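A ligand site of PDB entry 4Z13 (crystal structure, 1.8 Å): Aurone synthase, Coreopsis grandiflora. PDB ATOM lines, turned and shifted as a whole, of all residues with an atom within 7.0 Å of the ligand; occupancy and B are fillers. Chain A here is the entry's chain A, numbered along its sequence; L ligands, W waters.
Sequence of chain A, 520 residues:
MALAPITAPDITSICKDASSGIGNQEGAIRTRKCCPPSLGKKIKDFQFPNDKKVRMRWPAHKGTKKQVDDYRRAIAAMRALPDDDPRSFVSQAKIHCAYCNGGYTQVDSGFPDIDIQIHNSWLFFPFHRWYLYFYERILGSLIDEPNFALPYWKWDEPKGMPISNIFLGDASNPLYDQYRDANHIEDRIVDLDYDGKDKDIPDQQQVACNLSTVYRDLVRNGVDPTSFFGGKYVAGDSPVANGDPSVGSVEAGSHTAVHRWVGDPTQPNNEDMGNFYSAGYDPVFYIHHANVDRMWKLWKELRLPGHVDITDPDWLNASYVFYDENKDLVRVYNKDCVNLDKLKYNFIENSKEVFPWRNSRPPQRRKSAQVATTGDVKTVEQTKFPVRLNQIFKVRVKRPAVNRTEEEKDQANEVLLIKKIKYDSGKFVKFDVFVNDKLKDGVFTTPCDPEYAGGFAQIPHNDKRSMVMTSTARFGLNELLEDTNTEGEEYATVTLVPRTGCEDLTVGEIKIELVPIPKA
OE1 of Glu 157 binds W4 of the ligand (2.3 Å).
An oxygen (O3) of the ligand sits close to the side-chain amino group of Lys 62, 2.5 Å away.
O1 of the ligand lies close to NZ of Lys 352 (2.7 Å).
The side-chain amino group (NZ) of Lys 154 sits close to an oxygen (O19) of the ligand, at 2.7 Å.
NZ of Lys 154 sits close to OE1 of Glu 157 (3.5 Å).
The backbone NH (N) of Lys 352 lies within hydrogen-bond range of the side-chain amide oxygen (OD1) of Asn 350.
ND2 of Asn 350 lies within hydrogen-bond range of O of Val 354.
O23 of the ligand sits close to NZ of Lys 159 (3.0 Å).
The side-chain amide nitrogen (ND2) of Asn 350 sits close to an oxygen (O18) of the ligand, 3.0 Å away.
Merely in contact with the ligand: Pro 356 and Pro 158.
Hydrophobic or aromatic side chains that line the ligand: Pro 158 and Pro 356.
Of the 20 residues printed, 8 come within 4 Å of the ligand.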
ATOM      1  N   PRO A  59      31.808  23.835 -37.815  1.00  0.00           N
ATOM      2  CA  PRO A  59      30.572  23.059 -37.652  1.00  0.00           C
ATOM      3  C   PRO A  59      29.706  23.107 -38.906  1.00  0.00           C
ATOM      4  O   PRO A  59      29.442  24.199 -39.407  1.00  0.00           O
ATOM      5  CB  PRO A  59      29.869  23.733 -36.460  1.00  0.00           C
ATOM      6  CG  PRO A  59      30.885  24.580 -35.817  1.00  0.00           C
ATOM      7  CD  PRO A  59      31.880  24.969 -36.875  1.00  0.00           C
ATOM      8  N   HIS A  61      26.679  22.921 -39.533  1.00  0.00           N
ATOM      9  CA  HIS A  61      25.438  23.705 -39.480  1.00  0.00           C
ATOM     10  C   HIS A  61      25.660  25.210 -39.296  1.00  0.00           C
ATOM     11  O   HIS A  61      24.689  25.961 -39.209  1.00  0.00           O
ATOM     12  CB  HIS A  61      24.536  23.185 -38.349  1.00  0.00           C
ATOM     13  CG  HIS A  61      25.075  23.459 -36.977  1.00  0.00           C
ATOM     14  ND1 HIS A  61      26.235  22.908 -36.501  1.00  0.00           N
ATOM     15  CD2 HIS A  61      24.588  24.241 -35.970  1.00  0.00           C
ATOM     16  CE1 HIS A  61      26.448  23.330 -35.268  1.00  0.00           C
ATOM     17  NE2 HIS A  61      25.468  24.145 -34.928  1.00  0.00           N
ATOM     18  N   LYS A  62      26.917  25.645 -39.216  1.00  0.00           N
ATOM     19  CA  LYS A  62      27.213  27.060 -38.947  1.00  0.00           C
ATOM     20  C   LYS A  62      28.333  27.631 -39.823  1.00  0.00           C
ATOM     21  O   LYS A  62      29.082  28.505 -39.383  1.00  0.00           O
ATOM     22  CB  LYS A  62      27.595  27.264 -37.457  1.00  0.00           C
ATOM     23  CG  LYS A  62      26.497  26.903 -36.470  1.00  0.00           C
ATOM     24  CD  LYS A  62      26.114  28.070 -35.556  1.00  0.00           C
ATOM     25  CE  LYS A  62      27.059  28.215 -34.365  1.00  0.00           C
ATOM     26  NZ  LYS A  62      26.461  29.078 -33.312  1.00  0.00           N
ATOM     27  N   TYR A 152      32.783  19.814 -39.786  1.00  0.00           N
ATOM     28  CA  TYR A 152      32.606  18.625 -38.966  1.00  0.00           C
ATOM     29  C   TYR A 152      31.155  18.574 -38.500  1.00  0.00           C
ATOM     30  O   TYR A 152      30.520  19.603 -38.303  1.00  0.00           O
ATOM     31  CB  TYR A 152      33.572  18.608 -37.778  1.00  0.00           C
ATOM     32  CG  TYR A 152      33.466  19.732 -36.758  1.00  0.00           C
ATOM     33  CD1 TYR A 152      32.682  19.596 -35.613  1.00  0.00           C
ATOM     34  CD2 TYR A 152      34.208  20.888 -36.907  1.00  0.00           C
ATOM     35  CE1 TYR A 152      32.614  20.602 -34.666  1.00  0.00           C
ATOM     36  CE2 TYR A 152      34.150  21.903 -35.967  1.00  0.00           C
ATOM     37  CZ  TYR A 152      33.342  21.740 -34.843  1.00  0.00           C
ATOM     38  OH  TYR A 152      33.276  22.733 -33.882  1.00  0.00           O
ATOM     39  N   LYS A 154      28.809  18.362 -35.925  1.00  0.00           N
ATOM     40  CA  LYS A 154      28.822  18.586 -34.482  1.00  0.00           C
ATOM     41  C   LYS A 154      27.564  18.023 -33.857  1.00  0.00           C
ATOM     42  O   LYS A 154      26.710  18.780 -33.408  1.00  0.00           O
ATOM     43  CB  LYS A 154      28.979  20.082 -34.217  1.00  0.00           C
ATOM     44  CG  LYS A 154      29.534  20.431 -32.845  1.00  0.00           C
ATOM     45  CD  LYS A 154      29.700  21.918 -32.671  1.00  0.00           C
ATOM     46  CE  LYS A 154      30.192  22.263 -31.268  1.00  0.00           C
ATOM     47  NZ  LYS A 154      30.193  23.734 -31.035  1.00  0.00           N
ATOM     48  N   ASP A 156      27.373  16.635 -31.177  1.00  0.00           N
ATOM     49  CA  ASP A 156      27.483  16.949 -29.758  1.00  0.00           C
ATOM     50  C   ASP A 156      26.872  18.326 -29.417  1.00  0.00           C
ATOM     51  O   ASP A 156      26.858  18.730 -28.256  1.00  0.00           O
ATOM     52  CB  ASP A 156      28.955  16.891 -29.298  1.00  0.00           C
ATOM     53  CG  ASP A 156      29.897  17.700 -30.205  1.00  0.00           C
ATOM     54  OD1 ASP A 156      30.027  17.396 -31.410  1.00  0.00           O
ATOM     55  OD2 ASP A 156      30.561  18.618 -29.688  1.00  0.00           O
ATOM     56  N   GLU A 157      26.362  19.029 -30.431  1.00  0.00           N
ATOM     57  CA  GLU A 157      25.652  20.294 -30.265  1.00  0.00           C
ATOM     58  C   GLU A 157      24.207  20.106 -30.710  1.00  0.00           C
ATOM     59  O   GLU A 157      23.988  19.615 -31.801  1.00  0.00           O
ATOM     60  CB  GLU A 157      26.319  21.384 -31.098  1.00  0.00           C
ATOM     61  CG  GLU A 157      25.540  22.684 -31.221  1.00  0.00           C
ATOM     62  CD  GLU A 157      25.785  23.579 -30.031  1.00  0.00           C
ATOM     63  OE1 GLU A 157      26.934  24.037 -29.930  1.00  0.00           O
ATOM     64  OE2 GLU A 157      24.850  23.806 -29.229  1.00  0.00           O
ATOM     65  N   PRO A 158      23.213  20.516 -29.881  1.00  0.00           N
ATOM     66  CA  PRO A 158      21.817  20.261 -30.258  1.00  0.00           C
ATOM     67  C   PRO A 158      21.469  20.642 -31.687  1.00  0.00           C
ATOM     68  O   PRO A 158      20.913  19.817 -32.404  1.00  0.00           O
ATOM     69  CB  PRO A 158      21.042  21.109 -29.252  1.00  0.00           C
ATOM     70  CG  PRO A 158      21.890  21.056 -28.028  1.00  0.00           C
ATOM     71  CD  PRO A 158      23.313  21.050 -28.516  1.00  0.00           C
ATOM     72  N   LYS A 159      21.811  21.854 -32.133  1.00  0.00           N
ATOM     73  CA  LYS A 159      21.434  22.254 -33.487  1.00  0.00           C
ATOM     74  C   LYS A 159      22.317  21.554 -34.545  1.00  0.00           C
ATOM     75  O   LYS A 159      21.962  21.525 -35.725  1.00  0.00           O
ATOM     76  CB  LYS A 159      21.524  23.766 -33.638  1.00  0.00           C
ATOM     77  CG  LYS A 159      20.419  24.499 -32.865  1.00  0.00           C
ATOM     78  CD  LYS A 159      20.613  26.000 -32.861  1.00  0.00           C
ATOM     79  CE  LYS A 159      19.491  26.723 -32.096  1.00  0.00           C
ATOM     80  NZ  LYS A 159      19.800  28.157 -31.947  1.00  0.00           N
ATOM     81  N   LEU A 211      23.544  14.149 -25.661  1.00  0.00           N
ATOM     82  CA  LEU A 211      24.560  14.779 -24.836  1.00  0.00           C
ATOM     83  C   LEU A 211      25.119  13.783 -23.827  1.00  0.00           C
ATOM     84  O   LEU A 211      26.326  13.745 -23.593  1.00  0.00           O
ATOM     85  CB  LEU A 211      24.001  16.027 -24.128  1.00  0.00           C
ATOM     86  CG  LEU A 211      23.559  17.179 -25.033  1.00  0.00           C
ATOM     87  CD1 LEU A 211      22.933  18.267 -24.219  1.00  0.00           C
ATOM     88  CD2 LEU A 211      24.739  17.735 -25.847  1.00  0.00           C
ATOM     89  N   ARG A 294      37.685  14.998 -33.942  1.00  0.00           N
ATOM     90  CA  ARG A 294      37.608  16.033 -32.926  1.00  0.00           C
ATOM     91  C   ARG A 294      37.408  15.436 -31.525  1.00  0.00           C
ATOM     92  O   ARG A 294      37.969  15.945 -30.566  1.00  0.00           O
ATOM     93  CB  ARG A 294      36.507  17.025 -33.286  1.00  0.00           C
ATOM     94  CG  ARG A 294      36.249  18.147 -32.277  1.00  0.00           C
ATOM     95  CD  ARG A 294      35.246  19.166 -32.815  1.00  0.00           C
ATOM     96  NE  ARG A 294      34.782  20.014 -31.723  1.00  0.00           N
ATOM     97  CZ  ARG A 294      33.660  19.825 -31.039  1.00  0.00           C
ATOM     98  NH1 ARG A 294      32.836  18.819 -31.332  1.00  0.00           N
ATOM     99  NH2 ARG A 294      33.360  20.651 -30.042  1.00  0.00           N
ATOM    100  N   ILE A 348      37.242  24.821 -35.049  1.00  0.00           N
ATOM    101  CA  ILE A 348      36.624  25.977 -34.406  1.00  0.00           C
ATOM    102  C   ILE A 348      35.794  25.531 -33.201  1.00  0.00           C
ATOM    103  O   ILE A 348      34.842  24.764 -33.352  1.00  0.00           O
ATOM    104  CB  ILE A 348      35.728  26.757 -35.385  1.00  0.00           C
ATOM    105  CG1 ILE A 348      36.550  27.244 -36.592  1.00  0.00           C
ATOM    106  CG2 ILE A 348      35.049  27.946 -34.677  1.00  0.00           C
ATOM    107  CD1 ILE A 348      35.716  27.858 -37.705  1.00  0.00           C
ATOM    108  N   GLU A 349      36.151  26.016 -32.009  1.00  0.00           N
ATOM    109  CA  GLU A 349      35.420  25.677 -30.770  1.00  0.00           C
ATOM    110  C   GLU A 349      34.573  26.855 -30.272  1.00  0.00           C
ATOM    111  O   GLU A 349      34.611  27.939 -30.844  1.00  0.00           O
ATOM    112  CB  GLU A 349      36.404  25.242 -29.685  1.00  0.00           C
ATOM    113  CG  GLU A 349      37.252  24.025 -30.069  1.00  0.00           C
ATOM    114  CD  GLU A 349      36.433  22.756 -30.279  1.00  0.00           C
ATOM    115  OE1 GLU A 349      35.295  22.666 -29.790  1.00  0.00           O
ATOM    116  OE2 GLU A 349      36.944  21.845 -30.955  1.00  0.00           O
ATOM    117  N   ASN A 350      33.800  26.632 -29.208  1.00  0.00           N
ATOM    118  CA  ASN A 350      32.784  27.615 -28.817  1.00  0.00           C
ATOM    119  C   ASN A 350      33.321  28.827 -28.052  1.00  0.00           C
ATOM    120  O   ASN A 350      32.633  29.849 -27.951  1.00  0.00           O
ATOM    121  CB  ASN A 350      31.659  26.933 -28.004  1.00  0.00           C
ATOM    122  CG  ASN A 350      32.146  26.257 -26.715  1.00  0.00           C
ATOM    123  OD1 ASN A 350      33.266  26.477 -26.244  1.00  0.00           O
ATOM    124  ND2 ASN A 350      31.262  25.463 -26.117  1.00  0.00           N
ATOM    125  N   SER A 351      34.545  28.722 -27.553  1.00  0.00           N
ATOM    126  CA  SER A 351      35.152  29.769 -26.730  1.00  0.00           C
ATOM    127  C   SER A 351      34.265  30.076 -25.515  1.00  0.00           C
ATOM    128  O   SER A 351      34.103  31.226 -25.110  1.00  0.00           O
ATOM    129  CB  SER A 351      35.392  31.050 -27.540  1.00  0.00           C
ATOM    130  OG  SER A 351      36.231  31.950 -26.839  1.00  0.00           O
ATOM    131  N   LYS A 352      33.709  29.022 -24.938  1.00  0.00           N
ATOM    132  CA  LYS A 352      32.892  29.140 -23.743  1.00  0.00           C
ATOM    133  C   LYS A 352      33.484  28.343 -22.607  1.00  0.00           C
ATOM    134  O   LYS A 352      34.487  27.617 -22.785  1.00  0.00           O
ATOM    135  CB  LYS A 352      31.474  28.653 -24.017  1.00  0.00           C
ATOM    136  CG  LYS A 352      30.715  29.473 -25.030  1.00  0.00           C
ATOM    137  CD  LYS A 352      29.318  28.893 -25.187  1.00  0.00           C
ATOM    138  CE  LYS A 352      28.547  29.474 -26.366  1.00  0.00           C
ATOM    139  NZ  LYS A 352      27.182  28.815 -26.463  1.00  0.00           N
ATOM    140  N   VAL A 354      32.484  25.768 -21.130  1.00  0.00           N
ATOM    141  CA  VAL A 354      32.272  24.338 -21.067  1.00  0.00           C
ATOM    142  C   VAL A 354      31.685  23.755 -22.352  1.00  0.00           C
ATOM    143  O   VAL A 354      31.023  24.472 -23.115  1.00  0.00           O
ATOM    144  CB  VAL A 354      31.356  24.019 -19.870  1.00  0.00           C
ATOM    145  CG1 VAL A 354      29.908  24.287 -20.233  1.00  0.00           C
ATOM    146  CG2 VAL A 354      31.560  22.619 -19.403  1.00  0.00           C
ATOM    147  N   PHE A 355      31.916  22.465 -22.608  1.00  0.00           N
ATOM    148  CA  PHE A 355      31.223  21.782 -23.685  1.00  0.00           C
ATOM    149  C   PHE A 355      29.754  21.582 -23.274  1.00  0.00           C
ATOM    150  O   PHE A 355      29.468  21.392 -22.099  1.00  0.00           O
ATOM    151  CB  PHE A 355      31.849  20.429 -24.018  1.00  0.00           C
ATOM    152  CG  PHE A 355      33.330  20.491 -24.355  1.00  0.00           C
ATOM    153  CD1 PHE A 355      33.770  21.173 -25.472  1.00  0.00           C
ATOM    154  CD2 PHE A 355      34.267  19.827 -23.573  1.00  0.00           C
ATOM    155  CE1 PHE A 355      35.121  21.217 -25.796  1.00  0.00           C
ATOM    156  CE2 PHE A 355      35.616  19.878 -23.891  1.00  0.00           C
ATOM    157  CZ  PHE A 355      36.034  20.570 -25.010  1.00  0.00           C
ATOM    158  N   PRO A 356      28.830  21.621 -24.240  1.00  0.00           N
ATOM    159  CA  PRO A 356      27.407  21.471 -23.898  1.00  0.00           C
ATOM    160  C   PRO A 356      27.072  20.108 -23.263  1.00  0.00           C
ATOM    161  O   PRO A 356      26.049  19.989 -22.581  1.00  0.00           O
ATOM    162  CB  PRO A 356      26.699  21.633 -25.255  1.00  0.00           C
ATOM    163  CG  PRO A 356      27.756  21.393 -26.303  1.00  0.00           C
ATOM    164  CD  PRO A 356      29.041  21.866 -25.683  1.00  0.00           C
ATOM    165  N   TRP A 357      27.942  19.125 -23.444  1.00  0.00           N
ATOM    166  CA  TRP A 357      27.744  17.771 -22.914  1.00  0.00           C
ATOM    167  C   TRP A 357      28.597  17.488 -21.685  1.00  0.00           C
ATOM    168  O   TRP A 357      28.519  16.397 -21.116  1.00  0.00           O
ATOM    169  CB  TRP A 357      28.074  16.725 -23.997  1.00  0.00           C
ATOM    170  CG  TRP A 357      29.416  16.965 -24.616  1.00  0.00           C
ATOM    171  CD1 TRP A 357      29.676  17.684 -25.747  1.00  0.00           C
ATOM    172  CD2 TRP A 357      30.693  16.532 -24.114  1.00  0.00           C
ATOM    173  NE1 TRP A 357      31.021  17.729 -25.986  1.00  0.00           N
ATOM    174  CE2 TRP A 357      31.667  17.023 -25.005  1.00  0.00           C
ATOM    175  CE3 TRP A 357      31.098  15.768 -23.021  1.00  0.00           C
ATOM    176  CZ2 TRP A 357      33.033  16.770 -24.826  1.00  0.00           C
ATOM    177  CZ3 TRP A 357      32.460  15.535 -22.835  1.00  0.00           C
ATOM    178  CH2 TRP A 357      33.402  16.035 -23.743  1.00  0.00           C
HETATM  179  O1  LIG L   1      27.149  28.703 -29.172  1.00  0.00           O
HETATM  180  O2  LIG L   1      25.145  29.572 -30.500  1.00  0.00           O
HETATM  181  O3  LIG L   1      27.859  29.739 -31.404  1.00  0.00           O
HETATM  182  O4  LIG L   1      25.864  31.043 -28.458  1.00  0.00           O
HETATM  183  O5  LIG L   1      26.563  32.131 -30.997  1.00  0.00           O
HETATM  184  O6  LIG L   1      28.449  31.341 -29.211  1.00  0.00           O
HETATM  185  O7  LIG L   1      26.567  27.249 -31.325  1.00  0.00           O
HETATM  186  O8  LIG L   1      30.026  28.611 -29.925  1.00  0.00           O
HETATM  187  O9  LIG L   1      29.230  27.432 -32.290  1.00  0.00           O
HETATM  188  O10 LIG L   1      28.559  26.283 -30.003  1.00  0.00           O
HETATM  189  O11 LIG L   1      23.947  26.964 -30.391  1.00  0.00           O
HETATM  190  O12 LIG L   1      26.134  26.488 -28.703  1.00  0.00           O
HETATM  191  O13 LIG L   1      24.560  28.410 -28.235  1.00  0.00           O
HETATM  192  O14 LIG L   1      22.564  29.382 -29.359  1.00  0.00           O
HETATM  193  O15 LIG L   1      23.574  31.958 -29.765  1.00  0.00           O
HETATM  194  O16 LIG L   1      23.487  30.917 -27.212  1.00  0.00           O
HETATM  195  O17 LIG L   1      26.916  24.180 -26.858  1.00  0.00           O
HETATM  196  O18 LIG L   1      28.553  26.379 -27.112  1.00  0.00           O
HETATM  197  O19 LIG L   1      29.345  24.332 -28.498  1.00  0.00           O
HETATM  198  O20 LIG L   1      23.341  25.844 -28.248  1.00  0.00           O
HETATM  199  O21 LIG L   1      25.323  25.965 -25.857  1.00  0.00           O
HETATM  200  O22 LIG L   1      24.257  23.781 -26.533  1.00  0.00           O
HETATM  201  O23 LIG L   1      21.192  26.930 -29.577  1.00  0.00           O
HETATM  202  O24 LIG L   1      21.890  27.898 -27.122  1.00  0.00           O
HETATM  203 TE1  LIG L   1      25.560  27.803 -29.797  1.00  0.00          TE
HETATM  204  W1  LIG L   1      27.015  30.797 -29.989  1.00  0.00           W
HETATM  205  W2  LIG L   1      28.605  28.024 -30.786  1.00  0.00           W
HETATM  206  W3  LIG L   1      23.999  30.573 -28.828  1.00  0.00           W
HETATM  207  W4  LIG L   1      28.003  25.323 -28.307  1.00  0.00           W
HETATM  208  W5  LIG L   1      24.973  25.107 -27.261  1.00  0.00           W
HETATM  209  W6  LIG L   1      22.545  27.541 -28.686  1.00  0.00           W
HETATM  210  O   HOH W   1      22.629  23.980 -30.452  1.00  0.00           O
HETATM  211  O   HOH W   2      24.672  28.934 -25.331  1.00  0.00           O
HETATM  212  O   HOH W   3      31.578  22.527 -28.014  1.00  0.00           O
HETATM  213  O   HOH W   4      27.658  25.316 -24.169  1.00  0.00           O
HETATM  214  O   HOH W   5      28.491  34.478 -30.696  1.00  0.00           O
HETATM  215  O   HOH W   6      24.763  25.667 -32.533  1.00  0.00           O
HETATM  216  O   HOH W   7      32.621  29.591 -31.924  1.00  0.00           O
HETATM  217  O   HOH W   8      23.148  22.092 -24.670  1.00  0.00           O
HETATM  218  O   HOH W   9      29.792  30.971 -32.789  1.00  0.00           O
